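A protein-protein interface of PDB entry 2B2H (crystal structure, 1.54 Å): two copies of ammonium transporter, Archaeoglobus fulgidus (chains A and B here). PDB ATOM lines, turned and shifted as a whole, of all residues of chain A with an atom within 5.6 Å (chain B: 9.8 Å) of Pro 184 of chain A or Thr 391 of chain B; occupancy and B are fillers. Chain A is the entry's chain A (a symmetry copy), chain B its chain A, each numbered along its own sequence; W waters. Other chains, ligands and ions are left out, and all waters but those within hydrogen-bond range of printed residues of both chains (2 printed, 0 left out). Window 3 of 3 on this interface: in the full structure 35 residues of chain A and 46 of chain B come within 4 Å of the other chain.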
ATOM      1  N   GLY A  29      -4.254   2.272 -13.915  1.00  0.00           N
ATOM      2  CA  GLY A  29      -3.623   2.793 -12.719  1.00  0.00           C
ATOM      3  C   GLY A  29      -4.287   2.340 -11.433  1.00  0.00           C
ATOM      4  O   GLY A  29      -3.664   2.365 -10.375  1.00  0.00           O
ATOM      5  N   MET A  30      -5.548   1.919 -11.522  1.00  0.00           N
ATOM      6  CA  MET A  30      -6.296   1.475 -10.348  1.00  0.00           C
ATOM      7  C   MET A  30      -6.185  -0.017 -10.031  1.00  0.00           C
ATOM      8  O   MET A  30      -6.609  -0.455  -8.956  1.00  0.00           O
ATOM      9  CB  MET A  30      -7.770   1.851 -10.498  1.00  0.00           C
ATOM     10  CG  MET A  30      -8.025   3.348 -10.526  1.00  0.00           C
ATOM     11  SD  MET A  30      -9.781   3.737 -10.734  1.00  0.00           S
ATOM     12  CE  MET A  30      -9.964   3.592 -12.443  1.00  0.00           C
ATOM     13  N   VAL A  31      -5.643  -0.805 -10.956  1.00  0.00           N
ATOM     14  CA  VAL A  31      -5.491  -2.231 -10.695  1.00  0.00           C
ATOM     15  C   VAL A  31      -4.055  -2.520 -10.281  1.00  0.00           C
ATOM     16  O   VAL A  31      -3.201  -1.628 -10.266  1.00  0.00           O
ATOM     17  CB  VAL A  31      -5.857  -3.096 -11.932  1.00  0.00           C
ATOM     18  CG1 VAL A  31      -7.278  -2.778 -12.379  1.00  0.00           C
ATOM     19  CG2 VAL A  31      -4.865  -2.872 -13.063  1.00  0.00           C
ATOM     20  N   ARG A  33      -0.200  -4.019 -10.343  1.00  0.00           N
ATOM     21  CA  ARG A  33       0.877  -4.014 -11.313  1.00  0.00           C
ATOM     22  C   ARG A  33       0.850  -5.216 -12.249  1.00  0.00           C
ATOM     23  O   ARG A  33       1.096  -5.074 -13.451  1.00  0.00           O
ATOM     24  CB  ARG A  33       2.205  -3.938 -10.565  1.00  0.00           C
ATOM     25  CG  ARG A  33       3.425  -3.964 -11.446  1.00  0.00           C
ATOM     26  CD  ARG A  33       4.683  -3.808 -10.603  1.00  0.00           C
ATOM     27  NE  ARG A  33       5.869  -4.283 -11.308  1.00  0.00           N
ATOM     28  CZ  ARG A  33       7.106  -4.195 -10.832  1.00  0.00           C
ATOM     29  NH1 ARG A  33       7.324  -3.642  -9.646  1.00  0.00           N
ATOM     30  NH2 ARG A  33       8.125  -4.669 -11.536  1.00  0.00           N
ATOM     31  N   ILE A 182      -7.816  -3.885  -2.836  1.00  0.00           N
ATOM     32  CA  ILE A 182      -6.837  -3.854  -3.920  1.00  0.00           C
ATOM     33  C   ILE A 182      -6.300  -2.429  -4.078  1.00  0.00           C
ATOM     34  O   ILE A 182      -7.072  -1.496  -4.313  1.00  0.00           O
ATOM     35  CB  ILE A 182      -7.494  -4.291  -5.253  1.00  0.00           C
ATOM     36  CG1 ILE A 182      -8.256  -5.606  -5.057  1.00  0.00           C
ATOM     37  CG2 ILE A 182      -6.446  -4.416  -6.338  1.00  0.00           C
ATOM     38  CD1 ILE A 182      -7.423  -6.734  -4.512  1.00  0.00           C
ATOM     39  N   GLU A 183      -4.986  -2.256  -3.957  1.00  0.00           N
ATOM     40  CA  GLU A 183      -4.370  -0.929  -4.082  1.00  0.00           C
ATOM     41  C   GLU A 183      -4.028  -0.523  -5.524  1.00  0.00           C
ATOM     42  O   GLU A 183      -3.575  -1.337  -6.322  1.00  0.00           O
ATOM     43  CB  GLU A 183      -3.079  -0.851  -3.246  1.00  0.00           C
ATOM     44  CG  GLU A 183      -3.238  -1.023  -1.735  1.00  0.00           C
ATOM     45  CD  GLU A 183      -4.171   0.004  -1.110  1.00  0.00           C
ATOM     46  OE1 GLU A 183      -4.095   1.197  -1.480  1.00  0.00           O
ATOM     47  OE2 GLU A 183      -4.976  -0.386  -0.233  1.00  0.00           O
ATOM     48  N   PRO A 184      -4.242   0.752  -5.874  1.00  0.00           N
ATOM     49  CA  PRO A 184      -3.914   1.166  -7.240  1.00  0.00           C
ATOM     50  C   PRO A 184      -2.394   1.127  -7.393  1.00  0.00           C
ATOM     51  O   PRO A 184      -1.674   1.681  -6.560  1.00  0.00           O
ATOM     52  CB  PRO A 184      -4.468   2.586  -7.310  1.00  0.00           C
ATOM     53  CG  PRO A 184      -4.329   3.071  -5.890  1.00  0.00           C
ATOM     54  CD  PRO A 184      -4.794   1.874  -5.093  1.00  0.00           C
ATOM     55  N   HIS A 185      -1.899   0.476  -8.442  1.00  0.00           N
ATOM     56  CA  HIS A 185      -0.455   0.395  -8.626  1.00  0.00           C
ATOM     57  C   HIS A 185       0.171   1.715  -9.083  1.00  0.00           C
ATOM     58  O   HIS A 185       1.343   1.975  -8.809  1.00  0.00           O
ATOM     59  CB  HIS A 185      -0.085  -0.733  -9.609  1.00  0.00           C
ATOM     60  CG  HIS A 185      -0.017  -0.309 -11.047  1.00  0.00           C
ATOM     61  ND1 HIS A 185      -1.131  -0.221 -11.853  1.00  0.00           N
ATOM     62  CD2 HIS A 185       1.038   0.045 -11.821  1.00  0.00           C
ATOM     63  CE1 HIS A 185      -0.766   0.168 -13.063  1.00  0.00           C
ATOM     64  NE2 HIS A 185       0.545   0.338 -13.069  1.00  0.00           N
ATOM     65  N   SER A 186      -0.603   2.555  -9.765  1.00  0.00           N
ATOM     66  CA  SER A 186      -0.065   3.825 -10.243  1.00  0.00           C
ATOM     67  C   SER A 186      -1.122   4.901 -10.384  1.00  0.00           C
ATOM     68  O   SER A 186      -1.759   5.015 -11.429  1.00  0.00           O
ATOM     69  CB  SER A 186       0.626   3.620 -11.596  1.00  0.00           C
ATOM     70  OG  SER A 186       1.152   4.840 -12.085  1.00  0.00           O
ATOM     71  N   ILE A 187      -1.312   5.693  -9.336  1.00  0.00           N
ATOM     72  CA  ILE A 187      -2.295   6.763  -9.404  1.00  0.00           C
ATOM     73  C   ILE A 187      -1.924   7.754 -10.530  1.00  0.00           C
ATOM     74  O   ILE A 187      -2.807   8.255 -11.227  1.00  0.00           O
ATOM     75  CB  ILE A 187      -2.442   7.456  -8.025  1.00  0.00           C
ATOM     76  CG1 ILE A 187      -3.092   6.473  -7.041  1.00  0.00           C
ATOM     77  CG2 ILE A 187      -3.293   8.719  -8.141  1.00  0.00           C
ATOM     78  CD1 ILE A 187      -3.282   7.010  -5.644  1.00  0.00           C
ATOM     79  N   LEU A 247      -7.981  10.420  -6.625  1.00  0.00           N
ATOM     80  CA  LEU A 247      -8.869   9.487  -7.309  1.00  0.00           C
ATOM     81  C   LEU A 247     -10.311   9.940  -7.144  1.00  0.00           C
ATOM     82  O   LEU A 247     -11.101   9.883  -8.091  1.00  0.00           O
ATOM     83  CB  LEU A 247      -8.699   8.064  -6.751  1.00  0.00           C
ATOM     84  CG  LEU A 247      -7.330   7.415  -6.989  1.00  0.00           C
ATOM     85  CD1 LEU A 247      -7.338   5.972  -6.501  1.00  0.00           C
ATOM     86  CD2 LEU A 247      -6.997   7.462  -8.470  1.00  0.00           C
ATOM     87  N   ARG B  33       8.783  10.892  -5.103  1.00  0.00           N
ATOM     88  CA  ARG B  33       7.708   9.930  -5.238  1.00  0.00           C
ATOM     89  C   ARG B  33       6.586  10.133  -4.227  1.00  0.00           C
ATOM     90  O   ARG B  33       5.407  10.012  -4.574  1.00  0.00           O
ATOM     91  CB  ARG B  33       8.294   8.526  -5.123  1.00  0.00           C
ATOM     92  CG  ARG B  33       7.284   7.413  -5.206  1.00  0.00           C
ATOM     93  CD  ARG B  33       7.987   6.063  -5.156  1.00  0.00           C
ATOM     94  NE  ARG B  33       7.073   4.993  -4.766  1.00  0.00           N
ATOM     95  CZ  ARG B  33       7.408   3.709  -4.716  1.00  0.00           C
ATOM     96  NH1 ARG B  33       8.637   3.329  -5.035  1.00  0.00           N
ATOM     97  NH2 ARG B  33       6.516   2.804  -4.334  1.00  0.00           N
ATOM     98  N   VAL B  37       1.495  12.372  -6.358  1.00  0.00           N
ATOM     99  CA  VAL B  37       0.055  12.595  -6.482  1.00  0.00           C
ATOM    100  C   VAL B  37      -0.327  14.047  -6.144  1.00  0.00           C
ATOM    101  O   VAL B  37      -1.137  14.661  -6.839  1.00  0.00           O
ATOM    102  CB  VAL B  37      -0.742  11.626  -5.576  1.00  0.00           C
ATOM    103  CG1 VAL B  37      -2.214  12.022  -5.537  1.00  0.00           C
ATOM    104  CG2 VAL B  37      -0.611  10.219  -6.102  1.00  0.00           C
ATOM    105  N   ASP B 381       1.344  13.092  -0.343  1.00  0.00           N
ATOM    106  CA  ASP B 381       0.420  12.111  -0.911  1.00  0.00           C
ATOM    107  C   ASP B 381      -0.342  11.461   0.250  1.00  0.00           C
ATOM    108  O   ASP B 381      -1.568  11.379   0.236  1.00  0.00           O
ATOM    109  CB  ASP B 381       1.184  11.050  -1.701  1.00  0.00           C
ATOM    110  CG  ASP B 381       1.754  11.594  -2.997  1.00  0.00           C
ATOM    111  OD1 ASP B 381       1.705  12.828  -3.195  1.00  0.00           O
ATOM    112  OD2 ASP B 381       2.253  10.795  -3.818  1.00  0.00           O
ATOM    113  N   LEU B 382       0.396  11.008   1.260  1.00  0.00           N
ATOM    114  CA  LEU B 382      -0.207  10.393   2.439  1.00  0.00           C
ATOM    115  C   LEU B 382      -0.867  11.449   3.316  1.00  0.00           C
ATOM    116  O   LEU B 382      -2.050  11.349   3.646  1.00  0.00           O
ATOM    117  CB  LEU B 382       0.854   9.681   3.284  1.00  0.00           C
ATOM    118  CG  LEU B 382       0.831   8.153   3.381  1.00  0.00           C
ATOM    119  CD1 LEU B 382      -0.606   7.654   3.557  1.00  0.00           C
ATOM    120  CD2 LEU B 382       1.441   7.561   2.130  1.00  0.00           C
ATOM    121  N   GLU B 386      -3.966  11.113   1.611  1.00  0.00           N
ATOM    122  CA  GLU B 386      -4.090   9.756   2.117  1.00  0.00           C
ATOM    123  C   GLU B 386      -4.021   8.766   0.957  1.00  0.00           C
ATOM    124  O   GLU B 386      -4.808   7.821   0.874  1.00  0.00           O
ATOM    125  CB  GLU B 386      -5.400   9.586   2.886  1.00  0.00           C
ATOM    126  CG  GLU B 386      -5.416  10.355   4.187  1.00  0.00           C
ATOM    127  CD  GLU B 386      -6.577   9.972   5.075  1.00  0.00           C
ATOM    128  OE1 GLU B 386      -6.649  10.490   6.208  1.00  0.00           O
ATOM    129  OE2 GLU B 386      -7.417   9.156   4.642  1.00  0.00           O
ATOM    130  N   GLU B 387      -3.077   9.009   0.055  1.00  0.00           N
ATOM    131  CA  GLU B 387      -2.871   8.150  -1.096  1.00  0.00           C
ATOM    132  C   GLU B 387      -1.390   7.856  -1.246  1.00  0.00           C
ATOM    133  O   GLU B 387      -0.546   8.563  -0.695  1.00  0.00           O
ATOM    134  CB  GLU B 387      -3.388   8.822  -2.374  1.00  0.00           C
ATOM    135  CG  GLU B 387      -4.896   8.774  -2.534  1.00  0.00           C
ATOM    136  CD  GLU B 387      -5.390   9.504  -3.769  1.00  0.00           C
ATOM    137  OE1 GLU B 387      -6.483   9.150  -4.249  1.00  0.00           O
ATOM    138  OE2 GLU B 387      -4.709  10.433  -4.256  1.00  0.00           O
ATOM    139  N   VAL B 388      -1.086   6.797  -1.982  1.00  0.00           N
ATOM    140  CA  VAL B 388       0.286   6.406  -2.259  1.00  0.00           C
ATOM    141  C   VAL B 388       0.369   6.331  -3.779  1.00  0.00           C
ATOM    142  O   VAL B 388      -0.366   5.570  -4.416  1.00  0.00           O
ATOM    143  CB  VAL B 388       0.616   5.031  -1.642  1.00  0.00           C
ATOM    144  CG1 VAL B 388       2.035   4.626  -1.998  1.00  0.00           C
ATOM    145  CG2 VAL B 388       0.460   5.098  -0.120  1.00  0.00           C
ATOM    146  N   ALA B 389       1.250   7.140  -4.356  1.00  0.00           N
ATOM    147  CA  ALA B 389       1.406   7.203  -5.804  1.00  0.00           C
ATOM    148  C   ALA B 389       1.600   5.853  -6.489  1.00  0.00           C
ATOM    149  O   ALA B 389       0.852   5.493  -7.397  1.00  0.00           O
ATOM    150  CB  ALA B 389       2.564   8.130  -6.152  1.00  0.00           C
ATOM    151  N   TYR B 390       2.611   5.108  -6.056  1.00  0.00           N
ATOM    152  CA  TYR B 390       2.906   3.815  -6.662  1.00  0.00           C
ATOM    153  C   TYR B 390       3.030   2.677  -5.657  1.00  0.00           C
ATOM    154  O   TYR B 390       3.542   2.848  -4.552  1.00  0.00           O
ATOM    155  CB  TYR B 390       4.210   3.888  -7.462  1.00  0.00           C
ATOM    156  CG  TYR B 390       4.364   5.126  -8.317  1.00  0.00           C
ATOM    157  CD1 TYR B 390       4.974   6.276  -7.813  1.00  0.00           C
ATOM    158  CD2 TYR B 390       3.911   5.145  -9.634  1.00  0.00           C
ATOM    159  CE1 TYR B 390       5.130   7.420  -8.614  1.00  0.00           C
ATOM    160  CE2 TYR B 390       4.061   6.279 -10.438  1.00  0.00           C
ATOM    161  CZ  TYR B 390       4.670   7.405  -9.925  1.00  0.00           C
ATOM    162  OH  TYR B 390       4.823   8.505 -10.732  1.00  0.00           O
ATOM    163  N   THR B 391       2.560   1.510  -6.064  1.00  0.00           N
ATOM    164  CA  THR B 391       2.640   0.316  -5.243  1.00  0.00           C
ATOM    165  C   THR B 391       3.293  -0.750  -6.115  1.00  0.00           C
ATOM    166  O   THR B 391       2.543  -1.498  -6.781  1.00  0.00           O
ATOM    167  CB  THR B 391       1.240  -0.163  -4.787  1.00  0.00           C
ATOM    168  OG1 THR B 391       0.720   0.744  -3.802  1.00  0.00           O
ATOM    169  CG2 THR B 391       1.324  -1.563  -4.189  1.00  0.00           C
HETATM  170  O   HOH W   1      -1.212   3.042  -4.439  1.00  0.00           O
HETATM  171  O   HOH W   2       0.710  -3.567  -7.637  1.00  0.00           O
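OE1 of Glu 387 of chain B is in hydrogen-bond range of N of Leu 247 of chain A (3.1 Å). O of Ala 389 of chain B sits at hydrogen-bond distance from N of Ile 187 of chain A (2.9 Å). The backbone NH (N) of Thr 391 of chain B lies within hydrogen-bond range of the backbone carbonyl oxygen (O) of His 185 of chain A.
Water W1 lies within hydrogen-bond range of O of Pro 184 of chain A (2.6 Å), O of Val 388 of chain B (2.7 Å) and OG1 of Thr 391 of chain B (3.1 Å). Water W2 lies within hydrogen-bond range of N of Arg 33 of chain A (2.9 Å) and O of Thr 391 of chain B (2.9 Å).
Of the 11 printed residues of chain A, 5 touch a printed residue of chain B. Hydrophobic or aromatic side chains of chain A that line the printed part of chain B: His 185, Ile 187 and Leu 247. Hydrophobic or aromatic side chains of chain B that line the printed part of chain A: Val 37 and Tyr 390. Among the printed residues, 11 pairs touch across the chains. Among the printed residues, no Asp or Glu carboxylate lies within 4 Å of a Lys or Arg side-chain nitrogen of the other chain.
No residue of chain B comes within 4 Å of Glu 183 of chain A. Of the printed residues of chain B, Pro 184 of chain A touches Thr 391. Printed residues of chain B within 4 Å of Ser 186 of chain A: Ala 389 (3.4 Å) and Tyr 390 (3.6 Å). Printed residues of chain B within 4 Å of Ile 187 of chain A: Val 37, Glu 387, Val 388 and Ala 389. Printed residues of chain A within 4 Å of Val 37 of chain B: Ile 187 (3.7 Å). Printed residues of chain A within 4 Å of Glu 387 of chain B: Ile 187 and Leu 247. Printed residues of chain A within 4 Å of Tyr 390 of chain B: His 185 and Ser 186. Thr 391 of chain B touches two residues of chain A. The nearest residue of chain A that does not touch Thr 391 of chain B is Glu 183 of chain A (4.2 Å).
1 position is printed for both chains.
NH2 of Arg 33 of chain B sits at hydrogen-bond distance from O of Tyr 390 of chain B (3.0 Å). N of Val 37 of chain B lies within hydrogen-bond range of OD2 of Asp 381 of chain B (3.1 Å). N of Glu 387 of chain B sits at hydrogen-bond distance from O of Asp 381 of chain B, at 2.8 Å. The backbone NH (N) of Leu 382 of chain B lies within hydrogen-bond range of the backbone carbonyl oxygen (O) of Glu 387 of chain B (3.3 Å). The backbone carbonyl oxygen of Gly 29 of chain A is in hydrogen-bond range of the backbone NH of Ser 186 of chain A. ND1 of His 185 of chain A sits at hydrogen-bond distance from O of Val 31 of chain A, 3.0 Å away.
Among the printed residues, merely in contact across the chains: His 185 of chain A with Tyr 390 of chain B (3.2 Å), Ser 186 of chain A with Ala 389 of chain B (3.4 Å), Ile 187 of chain A with Val 388 of chain B (3.5 Å), Ser 186 of chain A with Tyr 390 of chain B (3.6 Å), Ile 187 of chain A with Val 37 of chain B (3.7 Å), Ile 187 of chain A with Glu 387 of chain B (3.7 Å), Pro 184 of chain A with Thr 391 of chain B (3.8 Å) and His 185 of chain A with Ala 389 of chain B (3.8 Å).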
